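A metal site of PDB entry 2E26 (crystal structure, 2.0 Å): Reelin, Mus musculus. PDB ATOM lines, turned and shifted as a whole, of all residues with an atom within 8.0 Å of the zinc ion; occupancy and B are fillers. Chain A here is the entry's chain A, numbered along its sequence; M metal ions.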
ATOM      1  N   CYS A 114     -27.790 -12.070 -17.314  1.00  0.00           N
ATOM      2  CA  CYS A 114     -26.375 -12.412 -17.140  1.00  0.00           C
ATOM      3  C   CYS A 114     -25.722 -12.713 -18.460  1.00  0.00           C
ATOM      4  O   CYS A 114     -26.023 -13.687 -19.128  1.00  0.00           O
ATOM      5  CB  CYS A 114     -26.200 -13.566 -16.140  1.00  0.00           C
ATOM      6  SG  CYS A 114     -26.556 -13.086 -14.419  1.00  0.00           S
ATOM      7  N   TYR A 115     -24.840 -11.806 -18.845  1.00  0.00           N
ATOM      8  CA  TYR A 115     -24.029 -12.072 -20.016  1.00  0.00           C
ATOM      9  C   TYR A 115     -22.591 -11.651 -19.672  1.00  0.00           C
ATOM     10  O   TYR A 115     -21.920 -12.352 -18.897  1.00  0.00           O
ATOM     11  CB  TYR A 115     -24.633 -11.407 -21.280  1.00  0.00           C
ATOM     12  CG  TYR A 115     -23.797 -11.615 -22.506  1.00  0.00           C
ATOM     13  CD1 TYR A 115     -23.409 -12.896 -22.900  1.00  0.00           C
ATOM     14  CD2 TYR A 115     -23.347 -10.520 -23.257  1.00  0.00           C
ATOM     15  CE1 TYR A 115     -22.590 -13.087 -23.988  1.00  0.00           C
ATOM     16  CE2 TYR A 115     -22.539 -10.721 -24.372  1.00  0.00           C
ATOM     17  CZ  TYR A 115     -22.167 -12.004 -24.718  1.00  0.00           C
ATOM     18  OH  TYR A 115     -21.355 -12.218 -25.803  1.00  0.00           O
ATOM     19  N   HIS A 116     -22.131 -10.524 -20.190  1.00  0.00           N
ATOM     20  CA  HIS A 116     -20.773 -10.063 -19.925  1.00  0.00           C
ATOM     21  C   HIS A 116     -20.825  -8.800 -19.068  1.00  0.00           C
ATOM     22  O   HIS A 116     -21.108  -7.706 -19.580  1.00  0.00           O
ATOM     23  CB  HIS A 116     -20.003  -9.847 -21.232  1.00  0.00           C
ATOM     24  CG  HIS A 116     -19.650 -11.125 -21.944  1.00  0.00           C
ATOM     25  ND1 HIS A 116     -18.665 -11.188 -22.913  1.00  0.00           N
ATOM     26  CD2 HIS A 116     -20.130 -12.382 -21.812  1.00  0.00           C
ATOM     27  CE1 HIS A 116     -18.571 -12.434 -23.362  1.00  0.00           C
ATOM     28  NE2 HIS A 116     -19.455 -13.168 -22.715  1.00  0.00           N
ATOM     29  N   SER A 126     -22.404 -14.932 -12.833  1.00  0.00           N
ATOM     30  CA  SER A 126     -21.166 -15.712 -12.904  1.00  0.00           C
ATOM     31  C   SER A 126     -20.957 -16.238 -14.316  1.00  0.00           C
ATOM     32  O   SER A 126     -21.194 -15.508 -15.270  1.00  0.00           O
ATOM     33  CB  SER A 126     -21.082 -16.802 -11.809  1.00  0.00           C
ATOM     34  OG  SER A 126     -22.327 -17.419 -11.557  1.00  0.00           O
ATOM     35  N   THR A 127     -20.492 -17.480 -14.456  1.00  0.00           N
ATOM     36  CA  THR A 127     -20.144 -17.987 -15.781  1.00  0.00           C
ATOM     37  C   THR A 127     -21.364 -18.256 -16.655  1.00  0.00           C
ATOM     38  O   THR A 127     -21.289 -18.143 -17.885  1.00  0.00           O
ATOM     39  CB  THR A 127     -19.253 -19.252 -15.688  1.00  0.00           C
ATOM     40  OG1 THR A 127     -19.890 -20.224 -14.856  1.00  0.00           O
ATOM     41  CG2 THR A 127     -17.876 -18.909 -15.072  1.00  0.00           C
ATOM     42  N   GLU A 128     -22.496 -18.597 -16.043  1.00  0.00           N
ATOM     43  CA  GLU A 128     -23.672 -18.992 -16.827  1.00  0.00           C
ATOM     44  C   GLU A 128     -24.358 -17.773 -17.425  1.00  0.00           C
ATOM     45  O   GLU A 128     -24.732 -16.849 -16.715  1.00  0.00           O
ATOM     46  CB  GLU A 128     -24.670 -19.806 -16.007  1.00  0.00           C
ATOM     47  CG  GLU A 128     -25.938 -20.182 -16.824  1.00  0.00           C
ATOM     48  CD  GLU A 128     -27.052 -20.771 -15.986  1.00  0.00           C
ATOM     49  OE1 GLU A 128     -27.077 -20.564 -14.755  1.00  0.00           O
ATOM     50  OE2 GLU A 128     -27.949 -21.428 -16.570  1.00  0.00           O
ATOM     51  N   HIS A 129     -24.494 -17.772 -18.751  1.00  0.00           N
ATOM     52  CA  HIS A 129     -25.238 -16.726 -19.436  1.00  0.00           C
ATOM     53  C   HIS A 129     -26.719 -17.081 -19.447  1.00  0.00           C
ATOM     54  O   HIS A 129     -27.101 -18.162 -19.896  1.00  0.00           O
ATOM     55  CB  HIS A 129     -24.730 -16.549 -20.870  1.00  0.00           C
ATOM     56  CG  HIS A 129     -23.286 -16.158 -20.968  1.00  0.00           C
ATOM     57  ND1 HIS A 129     -22.600 -15.600 -19.913  1.00  0.00           N
ATOM     58  CD2 HIS A 129     -22.409 -16.235 -21.992  1.00  0.00           C
ATOM     59  CE1 HIS A 129     -21.366 -15.348 -20.283  1.00  0.00           C
ATOM     60  NE2 HIS A 129     -21.224 -15.714 -21.549  1.00  0.00           N
ATOM     61  N   PRO A 301     -24.459 -10.816 -29.544  1.00  0.00           N
ATOM     62  CA  PRO A 301     -24.184 -12.108 -30.174  1.00  0.00           C
ATOM     63  C   PRO A 301     -25.318 -13.119 -30.023  1.00  0.00           C
ATOM     64  O   PRO A 301     -26.154 -12.991 -29.124  1.00  0.00           O
ATOM     65  CB  PRO A 301     -22.953 -12.617 -29.431  1.00  0.00           C
ATOM     66  CG  PRO A 301     -22.967 -11.902 -28.123  1.00  0.00           C
ATOM     67  CD  PRO A 301     -23.533 -10.544 -28.411  1.00  0.00           C
ATOM     68  N   LEU A 303     -25.930 -16.737 -28.827  1.00  0.00           N
ATOM     69  CA  LEU A 303     -25.298 -17.741 -28.003  1.00  0.00           C
ATOM     70  C   LEU A 303     -25.906 -19.115 -28.275  1.00  0.00           C
ATOM     71  O   LEU A 303     -27.128 -19.277 -28.359  1.00  0.00           O
ATOM     72  CB  LEU A 303     -25.443 -17.408 -26.511  1.00  0.00           C
ATOM     73  CG  LEU A 303     -25.121 -15.994 -26.003  1.00  0.00           C
ATOM     74  CD1 LEU A 303     -25.247 -15.901 -24.486  1.00  0.00           C
ATOM     75  CD2 LEU A 303     -23.747 -15.447 -26.458  1.00  0.00           C
ATOM     76  N   GLN A 305     -26.033 -22.713 -26.575  1.00  0.00           N
ATOM     77  CA  GLN A 305     -25.836 -23.295 -25.258  1.00  0.00           C
ATOM     78  C   GLN A 305     -26.544 -24.642 -25.190  1.00  0.00           C
ATOM     79  O   GLN A 305     -27.409 -24.930 -26.010  1.00  0.00           O
ATOM     80  CB  GLN A 305     -26.467 -22.382 -24.197  1.00  0.00           C
ATOM     81  CG  GLN A 305     -25.765 -21.016 -24.039  1.00  0.00           C
ATOM     82  CD  GLN A 305     -26.424 -20.175 -22.970  1.00  0.00           C
ATOM     83  OE1 GLN A 305     -27.565 -19.799 -23.112  1.00  0.00           O
ATOM     84  NE2 GLN A 305     -25.696 -19.890 -21.902  1.00  0.00           N
ATOM     85  N   LEU A 316     -22.218 -23.042 -22.229  1.00  0.00           N
ATOM     86  CA  LEU A 316     -21.922 -22.433 -23.518  1.00  0.00           C
ATOM     87  C   LEU A 316     -21.265 -23.400 -24.519  1.00  0.00           C
ATOM     88  O   LEU A 316     -20.289 -24.074 -24.183  1.00  0.00           O
ATOM     89  CB  LEU A 316     -21.020 -21.205 -23.303  1.00  0.00           C
ATOM     90  CG  LEU A 316     -20.730 -20.295 -24.503  1.00  0.00           C
ATOM     91  CD1 LEU A 316     -22.010 -19.644 -25.015  1.00  0.00           C
ATOM     92  CD2 LEU A 316     -19.700 -19.254 -24.113  1.00  0.00           C
ATOM     93  N   GLN A 318     -20.909 -22.051 -28.059  1.00  0.00           N
ATOM     94  CA  GLN A 318     -20.237 -21.048 -28.886  1.00  0.00           C
ATOM     95  C   GLN A 318     -21.017 -19.747 -28.853  1.00  0.00           C
ATOM     96  O   GLN A 318     -22.231 -19.769 -28.872  1.00  0.00           O
ATOM     97  CB  GLN A 318     -20.141 -21.538 -30.342  1.00  0.00           C
ATOM     98  CG  GLN A 318     -19.374 -20.603 -31.306  1.00  0.00           C
ATOM     99  CD  GLN A 318     -17.927 -20.365 -30.917  1.00  0.00           C
ATOM    100  OE1 GLN A 318     -17.172 -21.304 -30.661  1.00  0.00           O
ATOM    101  NE2 GLN A 318     -17.522 -19.088 -30.906  1.00  0.00           N
ATOM    102  N   GLU A 319     -20.303 -18.619 -28.778  1.00  0.00           N
ATOM    103  CA  GLU A 319     -20.917 -17.321 -29.040  1.00  0.00           C
ATOM    104  C   GLU A 319     -20.611 -16.911 -30.466  1.00  0.00           C
ATOM    105  O   GLU A 319     -19.468 -16.982 -30.904  1.00  0.00           O
ATOM    106  CB  GLU A 319     -20.379 -16.256 -28.082  1.00  0.00           C
ATOM    107  CG  GLU A 319     -20.621 -16.651 -26.634  1.00  0.00           C
ATOM    108  CD  GLU A 319     -20.192 -15.616 -25.618  1.00  0.00           C
ATOM    109  OE1 GLU A 319     -19.498 -14.634 -25.954  1.00  0.00           O
ATOM    110  OE2 GLU A 319     -20.557 -15.797 -24.443  1.00  0.00           O
ATOM    111  N   LEU A 321     -20.584 -13.774 -32.906  1.00  0.00           N
ATOM    112  CA  LEU A 321     -20.604 -12.311 -32.866  1.00  0.00           C
ATOM    113  C   LEU A 321     -20.983 -11.725 -34.224  1.00  0.00           C
ATOM    114  O   LEU A 321     -20.612 -12.264 -35.273  1.00  0.00           O
ATOM    115  CB  LEU A 321     -19.246 -11.750 -32.419  1.00  0.00           C
ATOM    116  CG  LEU A 321     -18.879 -11.697 -30.920  1.00  0.00           C
ATOM    117  CD1 LEU A 321     -19.018 -13.038 -30.231  1.00  0.00           C
ATOM    118  CD2 LEU A 321     -17.479 -11.123 -30.701  1.00  0.00           C
HETATM  119 ZN    ZN M   1     -19.725 -15.178 -22.843  1.00  0.00          ZN
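OE1 of Glu 319 is in hydrogen-bond range of OH of Tyr 115 (3.1 Å).
The backbone carbonyl oxygen (O) of Tyr 115 sits close to a ring nitrogen (ND1) of His 129.
The side-chain amide nitrogen (NE2) of Gln 305 lies within hydrogen-bond range of the backbone carbonyl oxygen (O) of His 129, 3.0 Å away.
Tyr 115 touches the zinc ion.
Four residues have an atom within 4 Å of the zinc ion: Tyr 115, His 116, His 129 and Glu 319.
The nearest printed residue that does not touch the zinc ion is Leu 316 (4.3 Å).
The side-chain carboxylate (OE2) of Glu 319 is bound to the zinc ion.
NE2 of His 116 binds the zinc ion (2.0 Å).
NE2 of His 129 is bound to the zinc ion, 2.1 Å away.
The zinc ion has three donor atoms within binding distance.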
